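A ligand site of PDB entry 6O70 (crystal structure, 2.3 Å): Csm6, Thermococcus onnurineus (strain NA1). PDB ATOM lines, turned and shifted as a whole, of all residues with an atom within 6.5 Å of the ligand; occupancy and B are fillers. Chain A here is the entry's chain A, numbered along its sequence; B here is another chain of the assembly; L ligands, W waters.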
ATOM      1  N   ARG A 335      12.247  29.128   7.772  1.00  0.00           N
ATOM      2  CA  ARG A 335      13.224  28.903   8.875  1.00  0.00           C
ATOM      3  C   ARG A 335      13.154  27.429   9.315  1.00  0.00           C
ATOM      4  O   ARG A 335      14.220  26.847   9.533  1.00  0.00           O
ATOM      5  CB  ARG A 335      13.030  29.851  10.062  1.00  0.00           C
ATOM      6  CG  ARG A 335      13.953  29.583  11.254  1.00  0.00           C
ATOM      7  CD  ARG A 335      15.444  29.571  10.957  1.00  0.00           C
ATOM      8  NE  ARG A 335      16.110  30.842  11.243  1.00  0.00           N
ATOM      9  CZ  ARG A 335      17.104  31.046  12.109  1.00  0.00           C
ATOM     10  NH1 ARG A 335      17.602  30.049  12.824  1.00  0.00           N
ATOM     11  NH2 ARG A 335      17.603  32.255  12.267  1.00  0.00           N
ATOM     12  N   VAL A 338      14.917  25.204   6.780  1.00  0.00           N
ATOM     13  CA  VAL A 338      16.402  25.375   6.895  1.00  0.00           C
ATOM     14  C   VAL A 338      16.938  24.590   8.106  1.00  0.00           C
ATOM     15  O   VAL A 338      17.983  23.949   7.963  1.00  0.00           O
ATOM     16  CB  VAL A 338      16.812  26.861   6.923  1.00  0.00           C
ATOM     17  CG1 VAL A 338      18.267  27.047   7.299  1.00  0.00           C
ATOM     18  CG2 VAL A 338      16.521  27.538   5.596  1.00  0.00           C
ATOM     19  N   GLU A 339      16.247  24.642   9.248  1.00  0.00           N
ATOM     20  CA  GLU A 339      16.653  23.961  10.506  1.00  0.00           C
ATOM     21  C   GLU A 339      16.580  22.446  10.310  1.00  0.00           C
ATOM     22  O   GLU A 339      17.541  21.755  10.698  1.00  0.00           O
ATOM     23  CB  GLU A 339      15.791  24.425  11.677  1.00  0.00           C
ATOM     24  CG  GLU A 339      15.957  25.900  12.010  1.00  0.00           C
ATOM     25  CD  GLU A 339      17.385  26.392  12.117  1.00  0.00           C
ATOM     26  OE1 GLU A 339      17.784  27.252  11.305  1.00  0.00           O
ATOM     27  OE2 GLU A 339      18.107  25.904  13.011  1.00  0.00           O
ATOM     28  N   LEU A 340      15.490  21.939   9.740  1.00  0.00           N
ATOM     29  CA  LEU A 340      15.318  20.491   9.443  1.00  0.00           C
ATOM     30  C   LEU A 340      16.378  20.038   8.440  1.00  0.00           C
ATOM     31  O   LEU A 340      16.981  18.976   8.660  1.00  0.00           O
ATOM     32  CB  LEU A 340      13.901  20.236   8.905  1.00  0.00           C
ATOM     33  CG  LEU A 340      12.779  20.258   9.938  1.00  0.00           C
ATOM     34  CD1 LEU A 340      11.423  20.225   9.254  1.00  0.00           C
ATOM     35  CD2 LEU A 340      12.928  19.107  10.914  1.00  0.00           C
ATOM     36  N   LYS A 342      19.360  21.134   7.915  1.00  0.00           N
ATOM     37  CA  LYS A 342      20.704  21.024   8.540  1.00  0.00           C
ATOM     38  C   LYS A 342      20.839  19.653   9.202  1.00  0.00           C
ATOM     39  O   LYS A 342      21.918  19.047   9.067  1.00  0.00           O
ATOM     40  CB  LYS A 342      20.930  22.182   9.524  1.00  0.00           C
ATOM     41  CG  LYS A 342      21.265  23.520   8.880  1.00  0.00           C
ATOM     42  CD  LYS A 342      21.527  24.616   9.881  1.00  0.00           C
ATOM     43  CE  LYS A 342      21.400  26.013   9.296  1.00  0.00           C
ATOM     44  NZ  LYS A 342      22.323  26.223   8.146  1.00  0.00           N
ATOM     45  N   ILE A 343      19.791  19.178   9.878  1.00  0.00           N
ATOM     46  CA  ILE A 343      19.741  17.833  10.526  1.00  0.00           C
ATOM     47  C   ILE A 343      19.697  16.766   9.432  1.00  0.00           C
ATOM     48  O   ILE A 343      20.339  15.711   9.609  1.00  0.00           O
ATOM     49  CB  ILE A 343      18.552  17.701  11.510  1.00  0.00           C
ATOM     50  CG1 ILE A 343      18.560  18.807  12.566  1.00  0.00           C
ATOM     51  CG2 ILE A 343      18.532  16.317  12.154  1.00  0.00           C
ATOM     52  CD1 ILE A 343      17.532  18.626  13.661  1.00  0.00           C
ATOM     53  N   LYS A 346      23.162  16.351   7.746  1.00  0.00           N
ATOM     54  CA  LYS A 346      24.037  15.625   8.694  1.00  0.00           C
ATOM     55  C   LYS A 346      23.761  14.122   8.602  1.00  0.00           C
ATOM     56  O   LYS A 346      24.730  13.345   8.597  1.00  0.00           O
ATOM     57  CB  LYS A 346      23.853  16.159  10.120  1.00  0.00           C
ATOM     58  CG  LYS A 346      24.764  15.533  11.159  1.00  0.00           C
ATOM     59  CD  LYS A 346      26.241  15.782  10.914  1.00  0.00           C
ATOM     60  CE  LYS A 346      26.606  17.244  10.835  1.00  0.00           C
ATOM     61  NZ  LYS A 346      28.072  17.445  10.973  1.00  0.00           N
ATOM     62  N   LEU A 362      21.302  15.297  19.977  1.00  0.00           N
ATOM     63  CA  LEU A 362      21.424  16.073  18.710  1.00  0.00           C
ATOM     64  C   LEU A 362      22.756  16.847  18.703  1.00  0.00           C
ATOM     65  O   LEU A 362      23.386  16.901  17.633  1.00  0.00           O
ATOM     66  CB  LEU A 362      20.199  16.996  18.609  1.00  0.00           C
ATOM     67  CG  LEU A 362      20.113  17.852  17.344  1.00  0.00           C
ATOM     68  CD1 LEU A 362      20.028  16.993  16.093  1.00  0.00           C
ATOM     69  CD2 LEU A 362      18.926  18.807  17.422  1.00  0.00           C
ATOM     70  N   LEU A 366      25.337  16.417  15.706  1.00  0.00           N
ATOM     71  CA  LEU A 366      25.804  17.542  14.853  1.00  0.00           C
ATOM     72  C   LEU A 366      27.258  17.936  15.131  1.00  0.00           C
ATOM     73  O   LEU A 366      27.783  18.713  14.344  1.00  0.00           O
ATOM     74  CB  LEU A 366      24.888  18.743  15.074  1.00  0.00           C
ATOM     75  CG  LEU A 366      23.411  18.518  14.781  1.00  0.00           C
ATOM     76  CD1 LEU A 366      22.588  19.663  15.311  1.00  0.00           C
ATOM     77  CD2 LEU A 366      23.187  18.353  13.303  1.00  0.00           C
ATOM     78  N   PHE A 368      29.116  19.217  18.486  1.00  0.00           N
ATOM     79  CA  PHE A 368      29.082  20.523  19.192  1.00  0.00           C
ATOM     80  C   PHE A 368      30.214  20.659  20.202  1.00  0.00           C
ATOM     81  O   PHE A 368      30.591  19.675  20.793  1.00  0.00           O
ATOM     82  CB  PHE A 368      27.782  20.584  20.009  1.00  0.00           C
ATOM     83  CG  PHE A 368      26.658  21.392  19.421  1.00  0.00           C
ATOM     84  CD1 PHE A 368      26.327  21.293  18.080  1.00  0.00           C
ATOM     85  CD2 PHE A 368      25.913  22.228  20.213  1.00  0.00           C
ATOM     86  CE1 PHE A 368      25.287  22.036  17.553  1.00  0.00           C
ATOM     87  CE2 PHE A 368      24.873  22.971  19.686  1.00  0.00           C
ATOM     88  CZ  PHE A 368      24.566  22.873  18.362  1.00  0.00           C
ATOM     89  N   ASN A 372      28.388  25.406  25.563  1.00  0.00           N
ATOM     90  CA  ASN A 372      27.066  25.816  26.123  1.00  0.00           C
ATOM     91  C   ASN A 372      26.099  24.625  26.133  1.00  0.00           C
ATOM     92  O   ASN A 372      25.672  24.212  25.039  1.00  0.00           O
ATOM     93  CB  ASN A 372      26.484  27.006  25.352  1.00  0.00           C
ATOM     94  CG  ASN A 372      25.636  27.917  26.222  1.00  0.00           C
ATOM     95  OD1 ASN A 372      25.935  28.125  27.400  1.00  0.00           O
ATOM     96  ND2 ASN A 372      24.598  28.492  25.642  1.00  0.00           N
ATOM     97  N   GLU A 374      23.451  24.876  28.580  1.00  0.00           N
ATOM     98  CA  GLU A 374      22.236  25.508  29.159  1.00  0.00           C
ATOM     99  C   GLU A 374      21.224  25.740  28.018  1.00  0.00           C
ATOM    100  O   GLU A 374      21.652  26.100  26.922  1.00  0.00           O
ATOM    101  CB  GLU A 374      22.572  26.772  29.943  1.00  0.00           C
ATOM    102  CG  GLU A 374      22.905  27.975  29.089  1.00  0.00           C
ATOM    103  CD  GLU A 374      23.598  29.117  29.826  1.00  0.00           C
ATOM    104  OE1 GLU A 374      24.456  29.790  29.217  1.00  0.00           O
ATOM    105  OE2 GLU A 374      23.273  29.326  31.019  1.00  0.00           O
ATOM    106  N   SER A 376      18.343  27.867  26.473  1.00  0.00           N
ATOM    107  CA  SER A 376      17.896  29.283  26.462  1.00  0.00           C
ATOM    108  C   SER A 376      16.644  29.433  25.591  1.00  0.00           C
ATOM    109  O   SER A 376      16.472  28.698  24.623  1.00  0.00           O
ATOM    110  CB  SER A 376      19.002  30.177  25.972  1.00  0.00           C
ATOM    111  OG  SER A 376      19.368  29.869  24.632  1.00  0.00           O
ATOM    112  N   ASN A 379      17.710  30.007  21.807  1.00  0.00           N
ATOM    113  CA  ASN A 379      18.098  28.834  20.982  1.00  0.00           C
ATOM    114  C   ASN A 379      16.879  27.952  20.709  1.00  0.00           C
ATOM    115  O   ASN A 379      16.824  27.421  19.587  1.00  0.00           O
ATOM    116  CB  ASN A 379      19.248  28.051  21.622  1.00  0.00           C
ATOM    117  CG  ASN A 379      20.553  28.823  21.583  1.00  0.00           C
ATOM    118  OD1 ASN A 379      20.757  29.664  20.717  1.00  0.00           O
ATOM    119  ND2 ASN A 379      21.429  28.558  22.532  1.00  0.00           N
ATOM    120  N   VAL A 380      15.954  27.795  21.665  1.00  0.00           N
ATOM    121  CA  VAL A 380      14.719  26.984  21.479  1.00  0.00           C
ATOM    122  C   VAL A 380      13.830  27.605  20.386  1.00  0.00           C
ATOM    123  O   VAL A 380      13.313  26.854  19.559  1.00  0.00           O
ATOM    124  CB  VAL A 380      13.945  26.793  22.798  1.00  0.00           C
ATOM    125  CG1 VAL A 380      12.528  26.259  22.576  1.00  0.00           C
ATOM    126  CG2 VAL A 380      14.696  25.901  23.770  1.00  0.00           C
ATOM    127  N   ALA A 382      14.617  30.118  18.053  1.00  0.00           N
ATOM    128  CA  ALA A 382      15.338  30.502  16.815  1.00  0.00           C
ATOM    129  C   ALA A 382      15.614  29.264  15.946  1.00  0.00           C
ATOM    130  O   ALA A 382      15.893  29.446  14.742  1.00  0.00           O
ATOM    131  CB  ALA A 382      16.629  31.212  17.160  1.00  0.00           C
ATOM    132  N   HIS A 383      15.559  28.064  16.534  1.00  0.00           N
ATOM    133  CA  HIS A 383      15.949  26.779  15.891  1.00  0.00           C
ATOM    134  C   HIS A 383      14.728  25.861  15.813  1.00  0.00           C
ATOM    135  O   HIS A 383      14.906  24.631  15.898  1.00  0.00           O
ATOM    136  CB  HIS A 383      17.145  26.153  16.634  1.00  0.00           C
ATOM    137  CG  HIS A 383      18.386  26.967  16.504  1.00  0.00           C
ATOM    138  ND1 HIS A 383      18.978  27.200  15.291  1.00  0.00           N
ATOM    139  CD2 HIS A 383      19.136  27.608  17.425  1.00  0.00           C
ATOM    140  CE1 HIS A 383      20.055  27.956  15.462  1.00  0.00           C
ATOM    141  NE2 HIS A 383      20.177  28.213  16.768  1.00  0.00           N
ATOM    142  N   ALA A 384      13.537  26.432  15.637  1.00  0.00           N
ATOM    143  CA  ALA A 384      12.257  25.729  15.419  1.00  0.00           C
ATOM    144  C   ALA A 384      12.052  24.676  16.514  1.00  0.00           C
ATOM    145  O   ALA A 384      11.480  23.605  16.214  1.00  0.00           O
ATOM    146  CB  ALA A 384      12.262  25.114  14.031  1.00  0.00           C
ATOM    147  N   LEU A 386      14.099  22.685  17.803  1.00  0.00           N
ATOM    148  CA  LEU A 386      15.011  21.524  17.603  1.00  0.00           C
ATOM    149  C   LEU A 386      16.363  21.859  18.243  1.00  0.00           C
ATOM    150  O   LEU A 386      17.385  21.908  17.525  1.00  0.00           O
ATOM    151  CB  LEU A 386      15.130  21.214  16.109  1.00  0.00           C
ATOM    152  CG  LEU A 386      13.811  21.068  15.359  1.00  0.00           C
ATOM    153  CD1 LEU A 386      14.053  20.620  13.921  1.00  0.00           C
ATOM    154  CD2 LEU A 386      12.879  20.090  16.052  1.00  0.00           C
ATOM    155  N   GLU A 387      16.363  22.102  19.547  1.00  0.00           N
ATOM    156  CA  GLU A 387      17.551  22.601  20.294  1.00  0.00           C
ATOM    157  C   GLU A 387      18.409  21.392  20.685  1.00  0.00           C
ATOM    158  O   GLU A 387      17.847  20.329  20.992  1.00  0.00           O
ATOM    159  CB  GLU A 387      17.073  23.465  21.465  1.00  0.00           C
ATOM    160  CG  GLU A 387      18.149  24.363  22.025  1.00  0.00           C
ATOM    161  CD  GLU A 387      19.077  23.707  23.027  1.00  0.00           C
ATOM    162  OE1 GLU A 387      18.715  22.636  23.552  1.00  0.00           O
ATOM    163  OE2 GLU A 387      20.161  24.281  23.280  1.00  0.00           O
ATOM    164  N   ALA A 388      19.728  21.550  20.647  1.00  0.00           N
ATOM    165  CA  ALA A 388      20.723  20.449  20.590  1.00  0.00           C
ATOM    166  C   ALA A 388      20.815  19.709  21.929  1.00  0.00           C
ATOM    167  O   ALA A 388      21.306  18.574  21.911  1.00  0.00           O
ATOM    168  CB  ALA A 388      22.068  21.000  20.164  1.00  0.00           C
ATOM    169  N   ASN A 389      20.356  20.308  23.017  1.00  0.00           N
ATOM    170  CA  ASN A 389      20.519  19.772  24.396  1.00  0.00           C
ATOM    171  C   ASN A 389      19.226  19.114  24.896  1.00  0.00           C
ATOM    172  O   ASN A 389      19.223  18.603  26.036  1.00  0.00           O
ATOM    173  CB  ASN A 389      20.957  20.863  25.377  1.00  0.00           C
ATOM    174  CG  ASN A 389      22.280  21.491  24.989  1.00  0.00           C
ATOM    175  OD1 ASN A 389      23.325  20.845  25.068  1.00  0.00           O
ATOM    176  ND2 ASN A 389      22.252  22.745  24.585  1.00  0.00           N
ATOM    177  N   LYS B 342      25.556  36.248  14.054  1.00  0.00           N
ATOM    178  CA  LYS B 342      26.517  35.530  13.167  1.00  0.00           C
ATOM    179  C   LYS B 342      27.441  36.541  12.488  1.00  0.00           C
ATOM    180  O   LYS B 342      28.651  36.295  12.444  1.00  0.00           O
ATOM    181  CB  LYS B 342      25.777  34.683  12.121  1.00  0.00           C
ATOM    182  CG  LYS B 342      24.993  33.508  12.675  1.00  0.00           C
ATOM    183  CD  LYS B 342      25.770  32.215  12.715  1.00  0.00           C
ATOM    184  CE  LYS B 342      24.984  31.067  13.333  1.00  0.00           C
ATOM    185  NZ  LYS B 342      23.807  30.701  12.516  1.00  0.00           N
HETATM  186  O1  LIG L   1      24.221  22.534  12.760  1.00  0.00           O
HETATM  187  P1  LIG L   1      23.303  23.669  13.176  1.00  0.00           P
HETATM  188  O2  LIG L   1      23.607  25.100  12.836  1.00  0.00           O
HETATM  189  O3  LIG L   1      23.065  23.540  14.751  1.00  0.00           O
HETATM  190  O4  LIG L   1      21.786  23.307  12.771  1.00  0.00           O
HETATM  191  C1  LIG L   1      20.995  22.814  13.852  1.00  0.00           C
HETATM  192  C2  LIG L   1      19.619  23.461  13.904  1.00  0.00           C
HETATM  193  O5  LIG L   1      19.647  24.421  14.983  1.00  0.00           O
HETATM  194  C3  LIG L   1      18.485  22.462  14.086  1.00  0.00           C
HETATM  195  O6  LIG L   1      18.629  21.663  15.261  1.00  0.00           O
HETATM  196  C4  LIG L   1      20.982  24.529  15.503  1.00  0.00           C
HETATM  197  N1  LIG L   1      21.029  24.608  16.976  1.00  0.00           N
HETATM  198  C5  LIG L   1      20.267  23.893  17.814  1.00  0.00           C
HETATM  199  N2  LIG L   1      20.559  24.193  19.099  1.00  0.00           N
HETATM  200  C6  LIG L   1      21.523  25.110  19.089  1.00  0.00           C
HETATM  201  C7  LIG L   1      22.295  25.834  20.112  1.00  0.00           C
HETATM  202  N3  LIG L   1      22.040  25.615  21.421  1.00  0.00           N
HETATM  203  N4  LIG L   1      23.229  26.715  19.708  1.00  0.00           N
HETATM  204  C8  LIG L   1      23.471  26.930  18.394  1.00  0.00           C
HETATM  205  N5  LIG L   1      22.808  26.294  17.409  1.00  0.00           N
HETATM  206  C9  LIG L   1      21.845  25.383  17.690  1.00  0.00           C
HETATM  207  C10 LIG L   1      21.709  23.254  15.100  1.00  0.00           C
HETATM  208  O   HOH W   1      20.382  26.716  24.243  1.00  0.00           O
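OE2 of Glu 387 lies within hydrogen-bond range of N3 of the ligand, at 3.0 Å.
The backbone carbonyl oxygen (O) of Leu 386 lies within hydrogen-bond range of an oxygen (O6) of the ligand (2.6 Å).
The backbone NH of Ala 388 is in hydrogen-bond range of a nitrogen (N2) of the ligand (3.2 Å).
The side-chain amide nitrogen of Asn 379 lies close to a nitrogen (N3) of the ligand (3.2 Å).
ND1 of His 383 is in hydrogen-bond range of O5 of the ligand (2.9 Å).
The side-chain carboxylate (OE1) of Glu 339 is in salt-bridge range of the guanidinium group (NH1) of Arg 335 (3.2 Å).
The side-chain hydroxyl of Ser 376 is in hydrogen-bond range of the side-chain amide nitrogen of Asn 379 (3.2 Å).
The backbone NH of Asn 389 sits at hydrogen-bond distance from the side-chain carboxylate of Glu 387 (2.9 Å).
The side-chain carboxylate (OE2) of Glu 339 is in hydrogen-bond range of a ring nitrogen (ND1) of His 383, 2.8 Å away.
O5 of the ligand sits close to OE2 of Glu 339, at 2.9 Å.
Lys 342 of chain A touches the ligand (CD to O4, 3.2 Å).
Ile 343 touches the ligand.
Leu 362 touches the ligand (CD2 to O6, 3.6 Å).
Leu 366 touches the ligand (CD1 to C10, 3.7 Å).
Phe 368 touches the ligand.
Hydrophobic or aromatic side chains that line the ligand: Ile 343, Leu 362, Leu 366, Phe 368, His 383, Leu 386 and Ala 388.
Of the 23 residues printed, 11 come within 4 Å of the ligand.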
